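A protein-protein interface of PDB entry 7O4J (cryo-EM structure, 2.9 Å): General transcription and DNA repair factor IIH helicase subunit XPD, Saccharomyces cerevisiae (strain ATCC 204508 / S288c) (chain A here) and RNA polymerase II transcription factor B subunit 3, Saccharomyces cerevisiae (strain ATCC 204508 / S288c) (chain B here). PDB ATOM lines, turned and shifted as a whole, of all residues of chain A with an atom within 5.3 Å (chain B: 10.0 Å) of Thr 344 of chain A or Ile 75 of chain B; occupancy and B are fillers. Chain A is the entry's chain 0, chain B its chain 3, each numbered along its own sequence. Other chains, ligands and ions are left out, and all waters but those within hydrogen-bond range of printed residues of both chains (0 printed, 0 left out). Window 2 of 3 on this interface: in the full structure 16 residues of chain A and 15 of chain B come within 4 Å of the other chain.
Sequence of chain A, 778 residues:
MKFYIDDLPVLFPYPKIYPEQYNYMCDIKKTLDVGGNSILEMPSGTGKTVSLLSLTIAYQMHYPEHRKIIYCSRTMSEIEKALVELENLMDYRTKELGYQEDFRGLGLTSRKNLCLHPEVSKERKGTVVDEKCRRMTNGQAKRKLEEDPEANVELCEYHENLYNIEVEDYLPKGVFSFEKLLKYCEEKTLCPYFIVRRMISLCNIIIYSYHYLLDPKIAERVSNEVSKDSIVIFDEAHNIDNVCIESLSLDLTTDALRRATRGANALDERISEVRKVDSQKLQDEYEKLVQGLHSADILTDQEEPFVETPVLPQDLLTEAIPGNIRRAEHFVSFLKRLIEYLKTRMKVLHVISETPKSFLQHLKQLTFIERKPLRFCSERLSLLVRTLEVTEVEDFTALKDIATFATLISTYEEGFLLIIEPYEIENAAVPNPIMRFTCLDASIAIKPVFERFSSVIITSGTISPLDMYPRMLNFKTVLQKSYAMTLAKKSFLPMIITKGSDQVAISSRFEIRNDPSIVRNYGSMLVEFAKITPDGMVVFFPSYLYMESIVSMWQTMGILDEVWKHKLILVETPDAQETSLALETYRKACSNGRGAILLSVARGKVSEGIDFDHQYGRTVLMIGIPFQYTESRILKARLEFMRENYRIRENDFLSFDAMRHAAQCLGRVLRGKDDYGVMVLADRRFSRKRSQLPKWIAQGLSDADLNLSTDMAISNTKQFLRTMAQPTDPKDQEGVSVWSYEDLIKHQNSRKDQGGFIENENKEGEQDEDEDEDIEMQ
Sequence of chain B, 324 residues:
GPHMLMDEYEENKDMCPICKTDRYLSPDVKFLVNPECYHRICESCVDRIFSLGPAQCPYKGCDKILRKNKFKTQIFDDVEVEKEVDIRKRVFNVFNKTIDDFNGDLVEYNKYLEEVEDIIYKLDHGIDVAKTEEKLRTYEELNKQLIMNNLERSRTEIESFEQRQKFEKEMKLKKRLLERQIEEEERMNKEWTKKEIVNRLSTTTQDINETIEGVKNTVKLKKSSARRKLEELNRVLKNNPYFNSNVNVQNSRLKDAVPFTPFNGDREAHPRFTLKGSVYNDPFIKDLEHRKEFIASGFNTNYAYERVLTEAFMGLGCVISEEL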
ATOM      1  N   ILE A 339      -0.399  23.803 -30.271  1.00  0.00           N
ATOM      2  CA  ILE A 339      -0.974  22.506 -29.926  1.00  0.00           C
ATOM      3  C   ILE A 339      -1.154  22.391 -28.420  1.00  0.00           C
ATOM      4  O   ILE A 339      -2.165  21.868 -27.937  1.00  0.00           O
ATOM      5  CB  ILE A 339      -0.095  21.369 -30.480  1.00  0.00           C
ATOM      6  CG1 ILE A 339      -0.100  21.392 -32.010  1.00  0.00           C
ATOM      7  CG2 ILE A 339      -0.583  20.023 -29.965  1.00  0.00           C
ATOM      8  CD1 ILE A 339       0.986  20.545 -32.639  1.00  0.00           C
ATOM      9  N   GLU A 340      -0.173  22.869 -27.652  1.00  0.00           N
ATOM     10  CA  GLU A 340      -0.282  22.811 -26.199  1.00  0.00           C
ATOM     11  C   GLU A 340      -1.477  23.613 -25.703  1.00  0.00           C
ATOM     12  O   GLU A 340      -2.194  23.172 -24.798  1.00  0.00           O
ATOM     13  CB  GLU A 340       1.008  23.322 -25.556  1.00  0.00           C
ATOM     14  CG  GLU A 340       2.206  22.414 -25.760  1.00  0.00           C
ATOM     15  CD  GLU A 340       1.997  21.030 -25.181  1.00  0.00           C
ATOM     16  OE1 GLU A 340       1.318  20.920 -24.139  1.00  0.00           O
ATOM     17  OE2 GLU A 340       2.510  20.054 -25.767  1.00  0.00           O
ATOM     18  N   TYR A 341      -1.706  24.795 -26.279  1.00  0.00           N
ATOM     19  CA  TYR A 341      -2.861  25.591 -25.880  1.00  0.00           C
ATOM     20  C   TYR A 341      -4.163  24.869 -26.198  1.00  0.00           C
ATOM     21  O   TYR A 341      -5.123  24.931 -25.421  1.00  0.00           O
ATOM     22  CB  TYR A 341      -2.830  26.953 -26.567  1.00  0.00           C
ATOM     23  CG  TYR A 341      -4.064  27.778 -26.295  1.00  0.00           C
ATOM     24  CD1 TYR A 341      -4.238  28.424 -25.080  1.00  0.00           C
ATOM     25  CD2 TYR A 341      -5.062  27.900 -27.249  1.00  0.00           C
ATOM     26  CE1 TYR A 341      -5.367  29.173 -24.826  1.00  0.00           C
ATOM     27  CE2 TYR A 341      -6.192  28.647 -27.006  1.00  0.00           C
ATOM     28  CZ  TYR A 341      -6.341  29.280 -25.795  1.00  0.00           C
ATOM     29  OH  TYR A 341      -7.472  30.023 -25.556  1.00  0.00           O
ATOM     30  N   LEU A 342      -4.226  24.193 -27.344  1.00  0.00           N
ATOM     31  CA  LEU A 342      -5.419  23.416 -27.664  1.00  0.00           C
ATOM     32  C   LEU A 342      -5.619  22.290 -26.659  1.00  0.00           C
ATOM     33  O   LEU A 342      -6.750  22.007 -26.250  1.00  0.00           O
ATOM     34  CB  LEU A 342      -5.314  22.856 -29.084  1.00  0.00           C
ATOM     35  CG  LEU A 342      -5.336  23.880 -30.222  1.00  0.00           C
ATOM     36  CD1 LEU A 342      -5.280  23.173 -31.565  1.00  0.00           C
ATOM     37  CD2 LEU A 342      -6.561  24.777 -30.141  1.00  0.00           C
ATOM     38  N   LYS A 343      -4.530  21.635 -26.251  1.00  0.00           N
ATOM     39  CA  LYS A 343      -4.641  20.542 -25.292  1.00  0.00           C
ATOM     40  C   LYS A 343      -5.143  21.034 -23.940  1.00  0.00           C
ATOM     41  O   LYS A 343      -6.000  20.394 -23.322  1.00  0.00           O
ATOM     42  CB  LYS A 343      -3.290  19.843 -25.139  1.00  0.00           C
ATOM     43  CG  LYS A 343      -3.023  18.779 -26.193  1.00  0.00           C
ATOM     44  CD  LYS A 343      -1.999  17.759 -25.722  1.00  0.00           C
ATOM     45  CE  LYS A 343      -0.582  18.241 -25.972  1.00  0.00           C
ATOM     46  NZ  LYS A 343       0.430  17.258 -25.496  1.00  0.00           N
ATOM     47  N   THR A 344      -4.625  22.167 -23.461  1.00  0.00           N
ATOM     48  CA  THR A 344      -5.040  22.664 -22.156  1.00  0.00           C
ATOM     49  C   THR A 344      -6.463  23.204 -22.173  1.00  0.00           C
ATOM     50  O   THR A 344      -7.052  23.394 -21.104  1.00  0.00           O
ATOM     51  CB  THR A 344      -4.073  23.745 -21.660  1.00  0.00           C
ATOM     52  OG1 THR A 344      -4.284  23.973 -20.261  1.00  0.00           O
ATOM     53  CG2 THR A 344      -4.264  25.048 -22.414  1.00  0.00           C
ATOM     54  N   ARG A 345      -7.025  23.453 -23.351  1.00  0.00           N
ATOM     55  CA  ARG A 345      -8.411  23.881 -23.480  1.00  0.00           C
ATOM     56  C   ARG A 345      -9.376  22.709 -23.588  1.00  0.00           C
ATOM     57  O   ARG A 345     -10.592  22.926 -23.631  1.00  0.00           O
ATOM     58  CB  ARG A 345      -8.565  24.790 -24.703  1.00  0.00           C
ATOM     59  CG  ARG A 345      -7.839  26.116 -24.573  1.00  0.00           C
ATOM     60  CD  ARG A 345      -8.597  27.080 -23.681  1.00  0.00           C
ATOM     61  NE  ARG A 345      -9.497  27.936 -24.450  1.00  0.00           N
ATOM     62  CZ  ARG A 345     -10.655  28.413 -24.003  1.00  0.00           C
ATOM     63  NH1 ARG A 345     -11.081  28.128 -22.780  1.00  0.00           N
ATOM     64  NH2 ARG A 345     -11.391  29.185 -24.787  1.00  0.00           N
ATOM     65  N   MET A 346      -8.868  21.481 -23.630  1.00  0.00           N
ATOM     66  CA  MET A 346      -9.693  20.285 -23.699  1.00  0.00           C
ATOM     67  C   MET A 346     -10.029  19.721 -22.325  1.00  0.00           C
ATOM     68  O   MET A 346     -10.701  18.688 -22.244  1.00  0.00           O
ATOM     69  CB  MET A 346      -8.983  19.208 -24.525  1.00  0.00           C
ATOM     70  CG  MET A 346      -8.899  19.511 -26.008  1.00  0.00           C
ATOM     71  SD  MET A 346     -10.356  18.971 -26.918  1.00  0.00           S
ATOM     72  CE  MET A 346      -9.733  19.009 -28.595  1.00  0.00           C
ATOM     73  N   LYS A 347      -9.582  20.370 -21.250  1.00  0.00           N
ATOM     74  CA  LYS A 347      -9.759  19.868 -19.895  1.00  0.00           C
ATOM     75  C   LYS A 347     -10.942  20.513 -19.184  1.00  0.00           C
ATOM     76  O   LYS A 347     -11.090  20.350 -17.968  1.00  0.00           O
ATOM     77  CB  LYS A 347      -8.479  20.084 -19.086  1.00  0.00           C
ATOM     78  CG  LYS A 347      -7.275  19.325 -19.623  1.00  0.00           C
ATOM     79  CD  LYS A 347      -6.081  19.418 -18.683  1.00  0.00           C
ATOM     80  CE  LYS A 347      -5.502  20.823 -18.647  1.00  0.00           C
ATOM     81  NZ  LYS A 347      -4.178  20.870 -17.967  1.00  0.00           N
ATOM     82  N   LEU A 366      -2.527  33.631 -22.815  1.00  0.00           N
ATOM     83  CA  LEU A 366      -1.768  32.534 -22.220  1.00  0.00           C
ATOM     84  C   LEU A 366      -0.442  32.341 -22.944  1.00  0.00           C
ATOM     85  O   LEU A 366       0.624  32.312 -22.319  1.00  0.00           O
ATOM     86  CB  LEU A 366      -2.596  31.251 -22.251  1.00  0.00           C
ATOM     87  CG  LEU A 366      -2.080  30.116 -21.367  1.00  0.00           C
ATOM     88  CD1 LEU A 366      -2.229  30.482 -19.898  1.00  0.00           C
ATOM     89  CD2 LEU A 366      -2.807  28.818 -21.678  1.00  0.00           C
ATOM     90  N   PHE B  31       1.466  19.595  -7.433  1.00  0.00           N
ATOM     91  CA  PHE B  31       2.833  19.830  -7.869  1.00  0.00           C
ATOM     92  C   PHE B  31       3.018  21.271  -8.335  1.00  0.00           C
ATOM     93  O   PHE B  31       2.063  21.970  -8.683  1.00  0.00           O
ATOM     94  CB  PHE B  31       3.210  18.866  -8.995  1.00  0.00           C
ATOM     95  CG  PHE B  31       3.163  17.420  -8.593  1.00  0.00           C
ATOM     96  CD1 PHE B  31       1.965  16.726  -8.587  1.00  0.00           C
ATOM     97  CD2 PHE B  31       4.319  16.755  -8.220  1.00  0.00           C
ATOM     98  CE1 PHE B  31       1.921  15.396  -8.217  1.00  0.00           C
ATOM     99  CE2 PHE B  31       4.281  15.425  -7.850  1.00  0.00           C
ATOM    100  CZ  PHE B  31       3.081  14.744  -7.848  1.00  0.00           C
ATOM    101  N   LEU B  32       4.275  21.707  -8.336  1.00  0.00           N
ATOM    102  CA  LEU B  32       4.634  23.053  -8.753  1.00  0.00           C
ATOM    103  C   LEU B  32       5.996  22.999  -9.429  1.00  0.00           C
ATOM    104  O   LEU B  32       6.753  22.037  -9.273  1.00  0.00           O
ATOM    105  CB  LEU B  32       4.654  24.022  -7.565  1.00  0.00           C
ATOM    106  CG  LEU B  32       3.325  24.234  -6.836  1.00  0.00           C
ATOM    107  CD1 LEU B  32       3.547  25.026  -5.558  1.00  0.00           C
ATOM    108  CD2 LEU B  32       2.314  24.934  -7.730  1.00  0.00           C
ATOM    109  N   VAL B  33       6.303  24.048 -10.188  1.00  0.00           N
ATOM    110  CA  VAL B  33       7.556  24.143 -10.926  1.00  0.00           C
ATOM    111  C   VAL B  33       8.215  25.477 -10.614  1.00  0.00           C
ATOM    112  O   VAL B  33       7.547  26.459 -10.273  1.00  0.00           O
ATOM    113  CB  VAL B  33       7.341  23.990 -12.448  1.00  0.00           C
ATOM    114  CG1 VAL B  33       6.790  22.611 -12.770  1.00  0.00           C
ATOM    115  CG2 VAL B  33       6.413  25.078 -12.971  1.00  0.00           C
ATOM    116  N   TYR B  38      12.804  24.133 -13.622  1.00  0.00           N
ATOM    117  CA  TYR B  38      11.607  23.453 -14.116  1.00  0.00           C
ATOM    118  C   TYR B  38      11.572  21.999 -13.656  1.00  0.00           C
ATOM    119  O   TYR B  38      11.387  21.068 -14.444  1.00  0.00           O
ATOM    120  CB  TYR B  38      11.524  23.545 -15.638  1.00  0.00           C
ATOM    121  CG  TYR B  38      11.049  24.890 -16.133  1.00  0.00           C
ATOM    122  CD1 TYR B  38       9.742  25.303 -15.927  1.00  0.00           C
ATOM    123  CD2 TYR B  38      11.911  25.748 -16.801  1.00  0.00           C
ATOM    124  CE1 TYR B  38       9.304  26.531 -16.375  1.00  0.00           C
ATOM    125  CE2 TYR B  38      11.482  26.978 -17.253  1.00  0.00           C
ATOM    126  CZ  TYR B  38      10.178  27.363 -17.038  1.00  0.00           C
ATOM    127  OH  TYR B  38       9.741  28.587 -17.483  1.00  0.00           O
ATOM    128  N   ARG B  40       9.659  19.297 -11.252  1.00  0.00           N
ATOM    129  CA  ARG B  40       8.396  19.064 -10.566  1.00  0.00           C
ATOM    130  C   ARG B  40       8.640  18.723  -9.103  1.00  0.00           C
ATOM    131  O   ARG B  40       9.559  17.970  -8.767  1.00  0.00           O
ATOM    132  CB  ARG B  40       7.626  17.934 -11.249  1.00  0.00           C
ATOM    133  CG  ARG B  40       7.135  18.280 -12.644  1.00  0.00           C
ATOM    134  CD  ARG B  40       6.361  17.129 -13.264  1.00  0.00           C
ATOM    135  NE  ARG B  40       5.101  16.873 -12.567  1.00  0.00           N
ATOM    136  CZ  ARG B  40       4.878  15.851 -11.744  1.00  0.00           C
ATOM    137  NH1 ARG B  40       5.828  14.959 -11.485  1.00  0.00           N
ATOM    138  NH2 ARG B  40       3.689  15.719 -11.171  1.00  0.00           N
ATOM    139  N   LYS B  72       5.417  28.248  -8.969  1.00  0.00           N
ATOM    140  CA  LYS B  72       4.150  28.518  -9.635  1.00  0.00           C
ATOM    141  C   LYS B  72       3.580  27.199 -10.143  1.00  0.00           C
ATOM    142  O   LYS B  72       4.198  26.139 -10.011  1.00  0.00           O
ATOM    143  CB  LYS B  72       4.330  29.527 -10.773  1.00  0.00           C
ATOM    144  CG  LYS B  72       5.145  29.004 -11.947  1.00  0.00           C
ATOM    145  CD  LYS B  72       5.270  30.048 -13.042  1.00  0.00           C
ATOM    146  CE  LYS B  72       6.085  29.530 -14.214  1.00  0.00           C
ATOM    147  NZ  LYS B  72       5.371  28.461 -14.964  1.00  0.00           N
ATOM    148  N   THR B  73       2.387  27.274 -10.729  1.00  0.00           N
ATOM    149  CA  THR B  73       1.705  26.101 -11.257  1.00  0.00           C
ATOM    150  C   THR B  73       1.982  25.972 -12.750  1.00  0.00           C
ATOM    151  O   THR B  73       1.910  26.958 -13.489  1.00  0.00           O
ATOM    152  CB  THR B  73       0.198  26.195 -11.008  1.00  0.00           C
ATOM    153  OG1 THR B  73      -0.052  26.304  -9.602  1.00  0.00           O
ATOM    154  CG2 THR B  73      -0.516  24.964 -11.554  1.00  0.00           C
ATOM    155  N   GLN B  74       2.296  24.755 -13.186  1.00  0.00           N
ATOM    156  CA  GLN B  74       2.551  24.509 -14.598  1.00  0.00           C
ATOM    157  C   GLN B  74       1.255  24.624 -15.389  1.00  0.00           C
ATOM    158  O   GLN B  74       0.233  24.041 -15.015  1.00  0.00           O
ATOM    159  CB  GLN B  74       3.171  23.127 -14.789  1.00  0.00           C
ATOM    160  CG  GLN B  74       3.935  22.964 -16.091  1.00  0.00           C
ATOM    161  CD  GLN B  74       4.508  21.572 -16.257  1.00  0.00           C
ATOM    162  OE1 GLN B  74       5.097  21.016 -15.330  1.00  0.00           O
ATOM    163  NE2 GLN B  74       4.338  20.999 -17.443  1.00  0.00           N
ATOM    164  N   ILE B  75       1.299  25.376 -16.487  1.00  0.00           N
ATOM    165  CA  ILE B  75       0.116  25.612 -17.308  1.00  0.00           C
ATOM    166  C   ILE B  75       0.018  24.531 -18.375  1.00  0.00           C
ATOM    167  O   ILE B  75      -0.983  23.813 -18.459  1.00  0.00           O
ATOM    168  CB  ILE B  75       0.154  27.012 -17.947  1.00  0.00           C
ATOM    169  CG1 ILE B  75       0.049  28.101 -16.873  1.00  0.00           C
ATOM    170  CG2 ILE B  75      -0.962  27.160 -18.969  1.00  0.00           C
ATOM    171  CD1 ILE B  75      -1.214  28.040 -16.030  1.00  0.00           C
ATOM    172  N   PHE B  76       1.056  24.410 -19.197  1.00  0.00           N
ATOM    173  CA  PHE B  76       1.084  23.430 -20.270  1.00  0.00           C
ATOM    174  C   PHE B  76       1.666  22.114 -19.772  1.00  0.00           C
ATOM    175  O   PHE B  76       2.574  22.088 -18.937  1.00  0.00           O
ATOM    176  CB  PHE B  76       1.903  23.950 -21.450  1.00  0.00           C
ATOM    177  CG  PHE B  76       1.411  25.257 -22.000  1.00  0.00           C
ATOM    178  CD1 PHE B  76       0.176  25.342 -22.620  1.00  0.00           C
ATOM    179  CD2 PHE B  76       2.181  26.402 -21.896  1.00  0.00           C
ATOM    180  CE1 PHE B  76      -0.280  26.543 -23.125  1.00  0.00           C
ATOM    181  CE2 PHE B  76       1.729  27.605 -22.400  1.00  0.00           C
ATOM    182  CZ  PHE B  76       0.498  27.675 -23.015  1.00  0.00           C
ATOM    183  N   ASP B  77       1.132  21.013 -20.297  1.00  0.00           N
ATOM    184  CA  ASP B  77       1.582  19.684 -19.903  1.00  0.00           C
ATOM    185  C   ASP B  77       2.972  19.350 -20.428  1.00  0.00           C
ATOM    186  O   ASP B  77       3.544  18.337 -20.013  1.00  0.00           O
ATOM    187  CB  ASP B  77       0.587  18.624 -20.383  1.00  0.00           C
ATOM    188  CG  ASP B  77       0.290  18.728 -21.867  1.00  0.00           C
ATOM    189  OD1 ASP B  77       1.250  18.789 -22.664  1.00  0.00           O
ATOM    190  OD2 ASP B  77      -0.902  18.751 -22.237  1.00  0.00           O
ATOM    191  N   ASP B  78       3.524  20.165 -21.323  1.00  0.00           N
ATOM    192  CA  ASP B  78       4.860  19.960 -21.869  1.00  0.00           C
ATOM    193  C   ASP B  78       5.808  20.942 -21.194  1.00  0.00           C
ATOM    194  O   ASP B  78       5.585  22.156 -21.239  1.00  0.00           O
ATOM    195  CB  ASP B  78       4.863  20.152 -23.387  1.00  0.00           C
ATOM    196  CG  ASP B  78       6.230  19.917 -24.007  1.00  0.00           C
ATOM    197  OD1 ASP B  78       7.227  20.477 -23.505  1.00  0.00           O
ATOM    198  OD2 ASP B  78       6.306  19.170 -25.005  1.00  0.00           O
ATOM    199  N   VAL B  79       6.862  20.413 -20.570  1.00  0.00           N
ATOM    200  CA  VAL B  79       7.795  21.263 -19.838  1.00  0.00           C
ATOM    201  C   VAL B  79       8.566  22.165 -20.794  1.00  0.00           C
ATOM    202  O   VAL B  79       8.800  23.344 -20.504  1.00  0.00           O
ATOM    203  CB  VAL B  79       8.743  20.402 -18.985  1.00  0.00           C
ATOM    204  CG1 VAL B  79       9.780  21.275 -18.294  1.00  0.00           C
ATOM    205  CG2 VAL B  79       7.952  19.595 -17.964  1.00  0.00           C
ATOM    206  N   VAL B  81       7.748  23.499 -23.661  1.00  0.00           N
ATOM    207  CA  VAL B  81       6.964  24.649 -24.097  1.00  0.00           C
ATOM    208  C   VAL B  81       6.830  25.666 -22.972  1.00  0.00           C
ATOM    209  O   VAL B  81       6.819  26.878 -23.220  1.00  0.00           O
ATOM    210  CB  VAL B  81       5.590  24.191 -24.616  1.00  0.00           C
ATOM    211  CG1 VAL B  81       4.742  25.392 -25.012  1.00  0.00           C
ATOM    212  CG2 VAL B  81       5.765  23.242 -25.792  1.00  0.00           C
ATOM    213  N   GLU B  82       6.729  25.203 -21.724  1.00  0.00           N
ATOM    214  CA  GLU B  82       6.673  26.128 -20.597  1.00  0.00           C
ATOM    215  C   GLU B  82       7.921  27.000 -20.551  1.00  0.00           C
ATOM    216  O   GLU B  82       7.838  28.213 -20.325  1.00  0.00           O
ATOM    217  CB  GLU B  82       6.513  25.353 -19.289  1.00  0.00           C
ATOM    218  CG  GLU B  82       5.106  24.847 -19.037  1.00  0.00           C
ATOM    219  CD  GLU B  82       4.159  25.951 -18.612  1.00  0.00           C
ATOM    220  OE1 GLU B  82       4.565  26.805 -17.797  1.00  0.00           O
ATOM    221  OE2 GLU B  82       3.009  25.967 -19.097  1.00  0.00           O
ATOM    222  N   LYS B  83       9.091  26.396 -20.762  1.00  0.00           N
ATOM    223  CA  LYS B  83      10.331  27.163 -20.769  1.00  0.00           C
ATOM    224  C   LYS B  83      10.320  28.209 -21.875  1.00  0.00           C
ATOM    225  O   LYS B  83      10.680  29.371 -21.654  1.00  0.00           O
ATOM    226  CB  LYS B  83      11.523  26.219 -20.934  1.00  0.00           C
ATOM    227  CG  LYS B  83      12.877  26.901 -20.820  1.00  0.00           C
ATOM    228  CD  LYS B  83      14.012  25.890 -20.870  1.00  0.00           C
ATOM    229  CE  LYS B  83      14.172  25.303 -22.263  1.00  0.00           C
ATOM    230  NZ  LYS B  83      15.428  24.517 -22.402  1.00  0.00           N
ATOM    231  N   VAL B  85       7.708  29.555 -23.459  1.00  0.00           N
ATOM    232  CA  VAL B  85       6.692  30.581 -23.241  1.00  0.00           C
ATOM    233  C   VAL B  85       7.155  31.577 -22.187  1.00  0.00           C
ATOM    234  O   VAL B  85       7.009  32.793 -22.357  1.00  0.00           O
ATOM    235  CB  VAL B  85       5.353  29.929 -22.855  1.00  0.00           C
ATOM    236  CG1 VAL B  85       4.371  30.980 -22.363  1.00  0.00           C
ATOM    237  CG2 VAL B  85       4.774  29.172 -24.039  1.00  0.00           C
ATOM    238  N   ASP B  86       7.717  31.084 -21.081  1.00  0.00           N
ATOM    239  CA  ASP B  86       8.176  31.985 -20.029  1.00  0.00           C
ATOM    240  C   ASP B  86       9.283  32.901 -20.533  1.00  0.00           C
ATOM    241  O   ASP B  86       9.286  34.102 -20.240  1.00  0.00           O
ATOM    242  CB  ASP B  86       8.649  31.179 -18.821  1.00  0.00           C
ATOM    243  CG  ASP B  86       7.506  30.508 -18.089  1.00  0.00           C
ATOM    244  OD1 ASP B  86       6.486  30.192 -18.737  1.00  0.00           O
ATOM    245  OD2 ASP B  86       7.626  30.295 -16.864  1.00  0.00           O
ATOM    246  N   LYS B  89       7.627  35.418 -22.649  1.00  0.00           N
ATOM    247  CA  LYS B  89       7.024  36.465 -21.832  1.00  0.00           C
ATOM    248  C   LYS B  89       8.078  37.443 -21.331  1.00  0.00           C
ATOM    249  O   LYS B  89       7.847  38.657 -21.311  1.00  0.00           O
ATOM    250  CB  LYS B  89       6.270  35.837 -20.660  1.00  0.00           C
ATOM    251  CG  LYS B  89       5.539  36.841 -19.778  1.00  0.00           C
ATOM    252  CD  LYS B  89       4.276  36.261 -19.134  1.00  0.00           C
ATOM    253  CE  LYS B  89       4.465  34.831 -18.629  1.00  0.00           C
ATOM    254  NZ  LYS B  89       3.235  34.314 -17.965  1.00  0.00           N
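The side-chain carboxylate (OE2) of Glu 340 of chain A lies within salt-bridge range of the side-chain amino group (NZ) of Lys 343 of chain A, at 3.5 Å.
The side-chain hydroxyl of Tyr 341 of chain A sits at hydrogen-bond distance from the guanidinium group of Arg 345 of chain A (3.1 Å).
O of Phe 76 of chain B lies within hydrogen-bond range of NE2 of Gln 74 of chain B, at 2.6 Å.
N of Ile 75 of chain B is in hydrogen-bond range of OE2 of Glu 82 of chain B, 3.2 Å away.
The backbone NH (N) of Phe 76 of chain B is in hydrogen-bond range of the side-chain carboxylate (OE2) of Glu 82 of chain B (2.5 Å).
The backbone NH of Val 81 of chain B is in hydrogen-bond range of the side-chain carboxylate of Asp 78 of chain B, at 3.1 Å.
Among the printed residues, merely in contact across the chains: Glu 340 of chain A with Phe 76 of chain B (3.7 Å), Glu 340 of chain A with Asp 78 of chain B (3.3 Å), Glu 340 of chain A with Val 81 of chain B (3.7 Å), Tyr 341 of chain A with Phe 76 of chain B (3.9 Å), Thr 344 of chain A with Ile 75 of chain B (3.8 Å), Leu 366 of chain A with Ile 75 of chain B (3.7 Å), Leu 366 of chain A with Phe 76 of chain B (3.7 Å) and Leu 366 of chain A with Val 85 of chain B (3.98 Å).
Of the 10 printed residues of chain A, 5 touch a printed residue of chain B.
Hydrophobic or aromatic side chains of chain A that line the printed part of chain B: Leu 366.
Of the 19 printed residues of chain B, 6 touch a printed residue of chain A.
Hydrophobic or aromatic side chains of chain B that line the printed part of chain A: Ile 75, Phe 76, Val 81 and Val 85.
Along chain B the printed residues that touch a printed residue of chain A span positions 75 to 85.
Among the printed residues, Asp or Glu carboxylates within 4 Å of a Lys or Arg side-chain nitrogen of the other chain: Lys 343 of chain A with Asp 77 of chain B (3.3 Å).
Thr 344 of chain A touches just one residue of chain B: Ile 75.
Ile 75 of chain B touches just these residues of chain A: Thr 344 (3.8 Å) and Leu 366 (3.7 Å).
Printed residues of chain B within 4 Å of Glu 340 of chain A: Phe 76, Asp 77, Asp 78 and Val 81.
Printed residues of chain A within 4 Å of Phe 76 of chain B: Glu 340, Tyr 341 and Leu 366.
Arg 345 of chain A touches none of the printed residues of chain B.
Leu 32 of chain B touches none of the printed residues of chain A.
The nearest residue of chain A that does not touch Ile 75 of chain B is Lys 347 of chain A (4.4 Å).
OD1 of Asp 77 of chain B sits close to OE1 of Glu 340 of chain A.
The side-chain amino group of Lys 343 of chain A is in salt-bridge range of the side-chain carboxylate of Asp 77 of chain B.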
